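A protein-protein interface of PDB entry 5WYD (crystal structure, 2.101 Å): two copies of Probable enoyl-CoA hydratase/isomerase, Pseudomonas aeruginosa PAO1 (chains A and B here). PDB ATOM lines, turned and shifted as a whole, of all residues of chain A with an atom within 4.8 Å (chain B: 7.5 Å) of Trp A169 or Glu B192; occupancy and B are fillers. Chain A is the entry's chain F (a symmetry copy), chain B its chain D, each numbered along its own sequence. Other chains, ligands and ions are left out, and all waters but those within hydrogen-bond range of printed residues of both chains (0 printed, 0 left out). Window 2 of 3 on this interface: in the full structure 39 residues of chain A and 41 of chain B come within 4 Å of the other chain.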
ATOM      1  N   VAL A 165      17.053  -3.915   2.299  1.00  0.00           N
ATOM      2  CA  VAL A 165      17.146  -3.458   3.688  1.00  0.00           C
ATOM      3  C   VAL A 165      16.869  -1.970   3.879  1.00  0.00           C
ATOM      4  O   VAL A 165      16.901  -1.491   5.023  1.00  0.00           O
ATOM      5  CB  VAL A 165      18.515  -3.828   4.282  1.00  0.00           C
ATOM      6  CG1 VAL A 165      18.725  -5.310   4.148  1.00  0.00           C
ATOM      7  CG2 VAL A 165      19.576  -3.124   3.531  1.00  0.00           C
ATOM      8  N   GLY A 166      16.619  -1.218   2.817  1.00  0.00           N
ATOM      9  CA  GLY A 166      16.412   0.209   2.961  1.00  0.00           C
ATOM     10  C   GLY A 166      17.711   0.979   2.812  1.00  0.00           C
ATOM     11  O   GLY A 166      18.809   0.452   2.976  1.00  0.00           O
ATOM     12  N   GLU A 167      17.571   2.261   2.484  1.00  0.00           N
ATOM     13  CA  GLU A 167      18.755   3.052   2.199  1.00  0.00           C
ATOM     14  C   GLU A 167      19.617   3.242   3.436  1.00  0.00           C
ATOM     15  O   GLU A 167      20.828   3.006   3.385  1.00  0.00           O
ATOM     16  CB  GLU A 167      18.332   4.387   1.569  1.00  0.00           C
ATOM     17  CG  GLU A 167      17.763   4.271   0.131  1.00  0.00           C
ATOM     18  CD  GLU A 167      17.525   5.636  -0.481  1.00  0.00           C
ATOM     19  OE1 GLU A 167      16.742   5.780  -1.462  1.00  0.00           O
ATOM     20  OE2 GLU A 167      18.189   6.574   0.005  1.00  0.00           O
ATOM     21  N   GLY A 168      19.009   3.578   4.575  1.00  0.00           N
ATOM     22  CA  GLY A 168      19.817   3.947   5.732  1.00  0.00           C
ATOM     23  C   GLY A 168      20.780   2.851   6.126  1.00  0.00           C
ATOM     24  O   GLY A 168      21.996   3.071   6.253  1.00  0.00           O
ATOM     25  N   TRP A 169      20.265   1.634   6.219  1.00  0.00           N
ATOM     26  CA  TRP A 169      21.112   0.514   6.569  1.00  0.00           C
ATOM     27  C   TRP A 169      22.099   0.202   5.463  1.00  0.00           C
ATOM     28  O   TRP A 169      23.252  -0.143   5.731  1.00  0.00           O
ATOM     29  CB  TRP A 169      20.234  -0.676   6.908  1.00  0.00           C
ATOM     30  CG  TRP A 169      20.021  -0.754   8.366  1.00  0.00           C
ATOM     31  CD1 TRP A 169      18.881  -0.488   9.050  1.00  0.00           C
ATOM     32  CD2 TRP A 169      20.993  -1.146   9.329  1.00  0.00           C
ATOM     33  NE1 TRP A 169      19.088  -0.688  10.394  1.00  0.00           N
ATOM     34  CE2 TRP A 169      20.380  -1.093  10.587  1.00  0.00           C
ATOM     35  CE3 TRP A 169      22.328  -1.541   9.243  1.00  0.00           C
ATOM     36  CZ2 TRP A 169      21.056  -1.430  11.755  1.00  0.00           C
ATOM     37  CZ3 TRP A 169      22.996  -1.871  10.399  1.00  0.00           C
ATOM     38  CH2 TRP A 169      22.360  -1.820  11.636  1.00  0.00           C
ATOM     39  N   ALA A 170      21.659   0.295   4.220  1.00  0.00           N
ATOM     40  CA  ALA A 170      22.549  -0.014   3.110  1.00  0.00           C
ATOM     41  C   ALA A 170      23.738   0.936   3.068  1.00  0.00           C
ATOM     42  O   ALA A 170      24.887   0.504   2.886  1.00  0.00           O
ATOM     43  CB  ALA A 170      21.769   0.040   1.799  1.00  0.00           C
ATOM     44  N   LYS A 171      23.488   2.225   3.276  1.00  0.00           N
ATOM     45  CA  LYS A 171      24.573   3.181   3.254  1.00  0.00           C
ATOM     46  C   LYS A 171      25.551   2.852   4.356  1.00  0.00           C
ATOM     47  O   LYS A 171      26.765   2.868   4.148  1.00  0.00           O
ATOM     48  CB  LYS A 171      23.991   4.567   3.443  1.00  0.00           C
ATOM     49  CG  LYS A 171      23.148   4.923   2.281  1.00  0.00           C
ATOM     50  CD  LYS A 171      22.508   6.242   2.486  1.00  0.00           C
ATOM     51  CE  LYS A 171      21.655   6.611   1.306  1.00  0.00           C
ATOM     52  NZ  LYS A 171      20.982   7.886   1.629  1.00  0.00           N
ATOM     53  N   ARG A 172      25.032   2.471   5.521  1.00  0.00           N
ATOM     54  CA  ARG A 172      25.899   2.191   6.658  1.00  0.00           C
ATOM     55  C   ARG A 172      26.858   1.059   6.332  1.00  0.00           C
ATOM     56  O   ARG A 172      28.032   1.096   6.695  1.00  0.00           O
ATOM     57  CB  ARG A 172      25.066   1.882   7.901  1.00  0.00           C
ATOM     58  CG  ARG A 172      25.871   2.104   9.153  1.00  0.00           C
ATOM     59  CD  ARG A 172      24.990   2.281  10.391  1.00  0.00           C
ATOM     60  NE  ARG A 172      24.638   1.043  11.070  1.00  0.00           N
ATOM     61  CZ  ARG A 172      25.160   0.671  12.242  1.00  0.00           C
ATOM     62  NH1 ARG A 172      26.038   1.456  12.858  1.00  0.00           N
ATOM     63  NH2 ARG A 172      24.816  -0.482  12.812  1.00  0.00           N
ATOM     64  N   MET A 173      26.375   0.020   5.677  1.00  0.00           N
ATOM     65  CA  MET A 173      27.283  -1.069   5.338  1.00  0.00           C
ATOM     66  C   MET A 173      28.294  -0.660   4.284  1.00  0.00           C
ATOM     67  O   MET A 173      29.466  -1.033   4.363  1.00  0.00           O
ATOM     68  CB  MET A 173      26.508  -2.285   4.885  1.00  0.00           C
ATOM     69  CG  MET A 173      25.566  -2.730   5.921  1.00  0.00           C
ATOM     70  SD  MET A 173      24.647  -4.111   5.235  1.00  0.00           S
ATOM     71  CE  MET A 173      25.959  -5.274   4.869  1.00  0.00           C
ATOM     72  N   VAL A 180      27.731  -6.889   9.180  1.00  0.00           N
ATOM     73  CA  VAL A 180      26.546  -7.239   9.958  1.00  0.00           C
ATOM     74  C   VAL A 180      26.583  -8.719  10.319  1.00  0.00           C
ATOM     75  O   VAL A 180      26.990  -9.559   9.510  1.00  0.00           O
ATOM     76  CB  VAL A 180      25.236  -6.881   9.213  1.00  0.00           C
ATOM     77  CG1 VAL A 180      25.139  -5.354   9.020  1.00  0.00           C
ATOM     78  CG2 VAL A 180      25.115  -7.641   7.893  1.00  0.00           C
ATOM     79  N   ILE A 188      17.137  -6.537   9.877  1.00  0.00           N
ATOM     80  CA  ILE A 188      17.008  -5.486   8.876  1.00  0.00           C
ATOM     81  C   ILE A 188      16.305  -5.952   7.618  1.00  0.00           C
ATOM     82  O   ILE A 188      16.047  -5.137   6.732  1.00  0.00           O
ATOM     83  CB  ILE A 188      18.395  -4.926   8.526  1.00  0.00           C
ATOM     84  CG1 ILE A 188      19.237  -5.975   7.818  1.00  0.00           C
ATOM     85  CG2 ILE A 188      19.106  -4.576   9.800  1.00  0.00           C
ATOM     86  CD1 ILE A 188      20.592  -5.461   7.414  1.00  0.00           C
ATOM     87  N   SER B 112      26.224  11.744   5.537  1.00  0.00           N
ATOM     88  CA  SER B 112      25.525  12.578   6.501  1.00  0.00           C
ATOM     89  C   SER B 112      24.894  11.689   7.559  1.00  0.00           C
ATOM     90  O   SER B 112      24.219  10.704   7.229  1.00  0.00           O
ATOM     91  CB  SER B 112      24.454  13.422   5.812  1.00  0.00           C
ATOM     92  OG  SER B 112      23.513  12.566   5.178  1.00  0.00           O
ATOM     93  N   ILE B 113      25.165  12.001   8.818  1.00  0.00           N
ATOM     94  CA  ILE B 113      24.591  11.297   9.957  1.00  0.00           C
ATOM     95  C   ILE B 113      23.882  12.303  10.836  1.00  0.00           C
ATOM     96  O   ILE B 113      24.455  13.338  11.177  1.00  0.00           O
ATOM     97  CB  ILE B 113      25.660  10.568  10.768  1.00  0.00           C
ATOM     98  CG1 ILE B 113      26.449   9.676   9.833  1.00  0.00           C
ATOM     99  CG2 ILE B 113      25.021   9.848  11.894  1.00  0.00           C
ATOM    100  CD1 ILE B 113      27.589   9.037  10.495  1.00  0.00           C
ATOM    101  N   ALA B 114      22.663  11.995  11.230  1.00  0.00           N
ATOM    102  CA  ALA B 114      21.896  12.858  12.110  1.00  0.00           C
ATOM    103  C   ALA B 114      21.936  12.273  13.515  1.00  0.00           C
ATOM    104  O   ALA B 114      21.644  11.089  13.715  1.00  0.00           O
ATOM    105  CB  ALA B 114      20.453  13.002  11.625  1.00  0.00           C
ATOM    106  N   ALA B 128      16.033  14.985   9.600  1.00  0.00           N
ATOM    107  CA  ALA B 128      16.764  13.777   9.941  1.00  0.00           C
ATOM    108  C   ALA B 128      16.659  12.752   8.831  1.00  0.00           C
ATOM    109  O   ALA B 128      17.609  11.999   8.574  1.00  0.00           O
ATOM    110  CB  ALA B 128      16.228  13.219  11.250  1.00  0.00           C
ATOM    111  N   CYS B 131      19.281  13.082   6.144  1.00  0.00           N
ATOM    112  CA  CYS B 131      20.586  12.501   6.410  1.00  0.00           C
ATOM    113  C   CYS B 131      20.610  11.015   6.066  1.00  0.00           C
ATOM    114  O   CYS B 131      19.606  10.307   6.150  1.00  0.00           O
ATOM    115  CB  CYS B 131      20.980  12.743   7.859  1.00  0.00           C
ATOM    116  SG  CYS B 131      20.981  14.508   8.297  1.00  0.00           S
ATOM    117  N   ASP B 132      21.778  10.560   5.644  1.00  0.00           N
ATOM    118  CA  ASP B 132      21.938   9.188   5.223  1.00  0.00           C
ATOM    119  C   ASP B 132      21.650   8.229   6.345  1.00  0.00           C
ATOM    120  O   ASP B 132      20.894   7.264   6.176  1.00  0.00           O
ATOM    121  CB  ASP B 132      23.351   9.014   4.718  1.00  0.00           C
ATOM    122  CG  ASP B 132      23.638   9.950   3.588  1.00  0.00           C
ATOM    123  OD1 ASP B 132      22.728  10.140   2.748  1.00  0.00           O
ATOM    124  OD2 ASP B 132      24.726  10.559   3.582  1.00  0.00           O
ATOM    125  N   ILE B 133      22.166   8.518   7.514  1.00  0.00           N
ATOM    126  CA  ILE B 133      22.037   7.608   8.634  1.00  0.00           C
ATOM    127  C   ILE B 133      21.522   8.411   9.804  1.00  0.00           C
ATOM    128  O   ILE B 133      21.794   9.613   9.934  1.00  0.00           O
ATOM    129  CB  ILE B 133      23.384   6.927   8.949  1.00  0.00           C
ATOM    130  CG1 ILE B 133      23.957   6.373   7.654  1.00  0.00           C
ATOM    131  CG2 ILE B 133      23.222   5.781   9.918  1.00  0.00           C
ATOM    132  CD1 ILE B 133      25.282   5.851   7.834  1.00  0.00           C
ATOM    133  N   ARG B 134      20.727   7.748  10.623  1.00  0.00           N
ATOM    134  CA  ARG B 134      20.127   8.350  11.795  1.00  0.00           C
ATOM    135  C   ARG B 134      20.535   7.560  13.020  1.00  0.00           C
ATOM    136  O   ARG B 134      20.559   6.327  12.987  1.00  0.00           O
ATOM    137  CB  ARG B 134      18.612   8.412  11.662  1.00  0.00           C
ATOM    138  CG  ARG B 134      18.137   9.382  10.594  1.00  0.00           C
ATOM    139  CD  ARG B 134      16.831   8.907   9.994  1.00  0.00           C
ATOM    140  NE  ARG B 134      17.061   7.600   9.405  1.00  0.00           N
ATOM    141  CZ  ARG B 134      17.680   7.433   8.252  1.00  0.00           C
ATOM    142  NH1 ARG B 134      18.121   8.494   7.575  1.00  0.00           N
ATOM    143  NH2 ARG B 134      17.884   6.210   7.792  1.00  0.00           N
ATOM    144  N   ILE B 135      20.981   8.280  14.044  1.00  0.00           N
ATOM    145  CA  ILE B 135      21.332   7.729  15.350  1.00  0.00           C
ATOM    146  C   ILE B 135      20.535   8.522  16.376  1.00  0.00           C
ATOM    147  O   ILE B 135      20.618   9.753  16.393  1.00  0.00           O
ATOM    148  CB  ILE B 135      22.839   7.848  15.643  1.00  0.00           C
ATOM    149  CG1 ILE B 135      23.689   7.207  14.551  1.00  0.00           C
ATOM    150  CG2 ILE B 135      23.153   7.242  16.994  1.00  0.00           C
ATOM    151  CD1 ILE B 135      25.215   7.315  14.824  1.00  0.00           C
ATOM    152  N   ALA B 136      19.796   7.841  17.251  1.00  0.00           N
ATOM    153  CA  ALA B 136      18.958   8.553  18.213  1.00  0.00           C
ATOM    154  C   ALA B 136      19.093   8.055  19.654  1.00  0.00           C
ATOM    155  O   ALA B 136      19.186   6.847  19.919  1.00  0.00           O
ATOM    156  CB  ALA B 136      17.477   8.450  17.793  1.00  0.00           C
ATOM    157  N   LEU B 164      11.858   4.511   3.964  1.00  0.00           N
ATOM    158  CA  LEU B 164      12.619   3.762   4.961  1.00  0.00           C
ATOM    159  C   LEU B 164      11.790   2.672   5.624  1.00  0.00           C
ATOM    160  O   LEU B 164      12.225   1.521   5.721  1.00  0.00           O
ATOM    161  CB  LEU B 164      13.155   4.701   6.035  1.00  0.00           C
ATOM    162  CG  LEU B 164      14.449   5.407   5.762  1.00  0.00           C
ATOM    163  CD1 LEU B 164      14.767   6.196   6.970  1.00  0.00           C
ATOM    164  CD2 LEU B 164      15.559   4.413   5.439  1.00  0.00           C
ATOM    165  N   ALA B 185      11.284   3.082  16.472  1.00  0.00           N
ATOM    166  CA  ALA B 185      11.890   3.556  15.231  1.00  0.00           C
ATOM    167  C   ALA B 185      13.001   2.631  14.759  1.00  0.00           C
ATOM    168  O   ALA B 185      13.150   2.371  13.558  1.00  0.00           O
ATOM    169  CB  ALA B 185      12.419   4.976  15.435  1.00  0.00           C
ATOM    170  N   LEU B 186      13.825   2.169  15.680  1.00  0.00           N
ATOM    171  CA  LEU B 186      14.847   1.211  15.317  1.00  0.00           C
ATOM    172  C   LEU B 186      14.220  -0.077  14.809  1.00  0.00           C
ATOM    173  O   LEU B 186      14.741  -0.710  13.882  1.00  0.00           O
ATOM    174  CB  LEU B 186      15.728   0.930  16.529  1.00  0.00           C
ATOM    175  CG  LEU B 186      16.675  -0.252  16.336  1.00  0.00           C
ATOM    176  CD1 LEU B 186      17.624   0.008  15.167  1.00  0.00           C
ATOM    177  CD2 LEU B 186      17.433  -0.565  17.608  1.00  0.00           C
ATOM    178  N   ILE B 188      11.300  -0.541  13.291  1.00  0.00           N
ATOM    179  CA  ILE B 188      10.742  -0.361  11.959  1.00  0.00           C
ATOM    180  C   ILE B 188      11.784   0.047  10.931  1.00  0.00           C
ATOM    181  O   ILE B 188      11.462   0.153   9.747  1.00  0.00           O
ATOM    182  CB  ILE B 188       9.627   0.689  11.976  1.00  0.00           C
ATOM    183  CG1 ILE B 188      10.195   2.042  12.350  1.00  0.00           C
ATOM    184  CG2 ILE B 188       8.613   0.303  12.986  1.00  0.00           C
ATOM    185  CD1 ILE B 188       9.120   3.103  12.389  1.00  0.00           C
ATOM    186  N   GLY B 189      13.008   0.315  11.339  1.00  0.00           N
ATOM    187  CA  GLY B 189      14.041   0.734  10.421  1.00  0.00           C
ATOM    188  C   GLY B 189      14.153   2.225  10.230  1.00  0.00           C
ATOM    189  O   GLY B 189      14.962   2.667   9.395  1.00  0.00           O
ATOM    190  N   LEU B 190      13.378   3.017  10.982  1.00  0.00           N
ATOM    191  CA  LEU B 190      13.464   4.468  10.851  1.00  0.00           C
ATOM    192  C   LEU B 190      14.856   4.971  11.255  1.00  0.00           C
ATOM    193  O   LEU B 190      15.437   5.833  10.584  1.00  0.00           O
ATOM    194  CB  LEU B 190      12.378   5.121  11.705  1.00  0.00           C
ATOM    195  CG  LEU B 190      12.286   6.639  11.721  1.00  0.00           C
ATOM    196  CD1 LEU B 190      12.044   7.085  10.300  1.00  0.00           C
ATOM    197  CD2 LEU B 190      11.187   7.152  12.635  1.00  0.00           C
ATOM    198  N   VAL B 191      15.417   4.421  12.330  1.00  0.00           N
ATOM    199  CA  VAL B 191      16.736   4.787  12.824  1.00  0.00           C
ATOM    200  C   VAL B 191      17.608   3.536  12.788  1.00  0.00           C
ATOM    201  O   VAL B 191      17.171   2.447  13.181  1.00  0.00           O
ATOM    202  CB  VAL B 191      16.672   5.399  14.237  1.00  0.00           C
ATOM    203  CG1 VAL B 191      15.900   6.701  14.196  1.00  0.00           C
ATOM    204  CG2 VAL B 191      16.094   4.426  15.255  1.00  0.00           C
ATOM    205  N   GLU B 192      18.805   3.679  12.229  1.00  0.00           N
ATOM    206  CA  GLU B 192      19.720   2.549  12.124  1.00  0.00           C
ATOM    207  C   GLU B 192      20.255   2.080  13.477  1.00  0.00           C
ATOM    208  O   GLU B 192      20.553   0.895  13.638  1.00  0.00           O
ATOM    209  CB  GLU B 192      20.855   2.859  11.148  1.00  0.00           C
ATOM    210  CG  GLU B 192      20.403   2.944   9.682  1.00  0.00           C
ATOM    211  CD  GLU B 192      19.485   4.103   9.366  1.00  0.00           C
ATOM    212  OE1 GLU B 192      19.823   5.256   9.731  1.00  0.00           O
ATOM    213  OE2 GLU B 192      18.414   3.859   8.764  1.00  0.00           O
ATOM    214  N   GLN B 193      20.500   2.990  14.421  1.00  0.00           N
ATOM    215  CA  GLN B 193      21.074   2.579  15.704  1.00  0.00           C
ATOM    216  C   GLN B 193      20.446   3.317  16.875  1.00  0.00           C
ATOM    217  O   GLN B 193      19.994   4.453  16.740  1.00  0.00           O
ATOM    218  CB  GLN B 193      22.593   2.806  15.712  1.00  0.00           C
ATOM    219  CG  GLN B 193      23.279   2.604  17.044  1.00  0.00           C
ATOM    220  CD  GLN B 193      24.727   2.934  16.975  1.00  0.00           C
ATOM    221  OE1 GLN B 193      25.241   3.272  15.918  1.00  0.00           O
ATOM    222  NE2 GLN B 193      25.392   2.890  18.112  1.00  0.00           N
ATOM    223  N   VAL B 194      20.481   2.685  18.049  1.00  0.00           N
ATOM    224  CA  VAL B 194      19.945   3.273  19.276  1.00  0.00           C
ATOM    225  C   VAL B 194      21.108   3.489  20.232  1.00  0.00           C
ATOM    226  O   VAL B 194      22.025   2.660  20.302  1.00  0.00           O
ATOM    227  CB  VAL B 194      18.849   2.403  19.916  1.00  0.00           C
ATOM    228  CG1 VAL B 194      19.372   1.013  20.152  1.00  0.00           C
ATOM    229  CG2 VAL B 194      18.370   3.021  21.217  1.00  0.00           C
ATOM    230  N   LEU B 207      31.310   7.545  14.345  1.00  0.00           N
ATOM    231  CA  LEU B 207      31.006   6.926  13.054  1.00  0.00           C
ATOM    232  C   LEU B 207      31.468   7.804  11.897  1.00  0.00           C
ATOM    233  O   LEU B 207      32.062   7.308  10.936  1.00  0.00           O
ATOM    234  CB  LEU B 207      29.503   6.661  12.935  1.00  0.00           C
ATOM    235  CG  LEU B 207      28.950   5.906  11.717  1.00  0.00           C
ATOM    236  CD1 LEU B 207      29.669   4.584  11.493  1.00  0.00           C
ATOM    237  CD2 LEU B 207      27.445   5.682  11.819  1.00  0.00           C
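Gly A168 touches Asp B132. NH2 of Arg B134 touches CA of Gly A168 (3.6 Å). Gly A168 touches Leu B164. CA of Gly A168 touches OE2 of Glu B192, at 3.3 Å. CZ2 of Trp A169 touches O of Glu B192 (3.0 Å). Arg A172 touches Ile B133. Arg A172 touches Gln B193.
Of chain B, only Glu B192 (3.0 Å) comes within 4 Å of Trp A169. Of the printed residues of chain B, Lys A171 touches Asp B132 (3.1 Å). Of the printed residues of chain B, Arg A172 touches Ile B133 (3.9 Å) and Gln B193 (3.6 Å). Ala B128 touches none of the printed residues of chain A. Printed residues of chain A within 4 Å of Ile B133: Arg A172. Of the printed residues of chain A, Arg B134 touches Gly A168. Ile B135 touches none of the printed residues of chain A. Of chain A, only Gly A168 (3.3 Å) and Trp A169 (3.0 Å) come within 4 Å of Glu B192. Printed residues of chain A within 4 Å of Gln B193: Arg A172 (3.6 Å). The nearest residue of chain B that does not touch Trp A169 is Val B191 (4.6 Å). The nearest printed residue of chain A that does not touch Gln B193 is Trp A169 (5.2 Å).
O of Ser B112 lies within hydrogen-bond range of N of Ile B133, at 3.0 Å. The guanidinium group (NH1) of Arg B134 lies within hydrogen-bond range of the backbone carbonyl oxygen (O) of Asp B132 (3.3 Å). OE2 of Glu A167 lies within salt-bridge range of NZ of Lys A171, 3.5 Å away. The backbone carbonyl oxygen (O) of Leu B190 lies within hydrogen-bond range of the guanidinium group (NE) of Arg B134, at 2.7 Å. The side-chain hydroxyl (OG) of Ser B112 sits at hydrogen-bond distance from the backbone NH (N) of Asp B132 (2.7 Å). The guanidinium group (NH2) of Arg B134 is in salt-bridge range of the side-chain carboxylate (OE2) of Glu B192 (2.6 Å).
Position printed for both chains: 188.
The side-chain carboxylate (OD1) of Asp B132 lies within salt-bridge range of the side-chain amino group (NZ) of Lys A171 (3.1 Å).
Of the 11 printed residues of chain A, 4 touch a printed residue of chain B. Printed residues of chain A that touch a printed residue of chain B: Gly A168, Trp A169, Lys A171 and Arg A172. Hydrophobic or aromatic side chains of chain A that line the printed part of chain B: Trp A169. Along chain B the printed residues that touch a printed residue of chain A span positions 132 to 193. Among the printed residues, Asp or Glu carboxylates within 4 Å of a Lys or Arg side-chain nitrogen of the other chain: Lys A171 with Asp B132 (3.1 Å).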
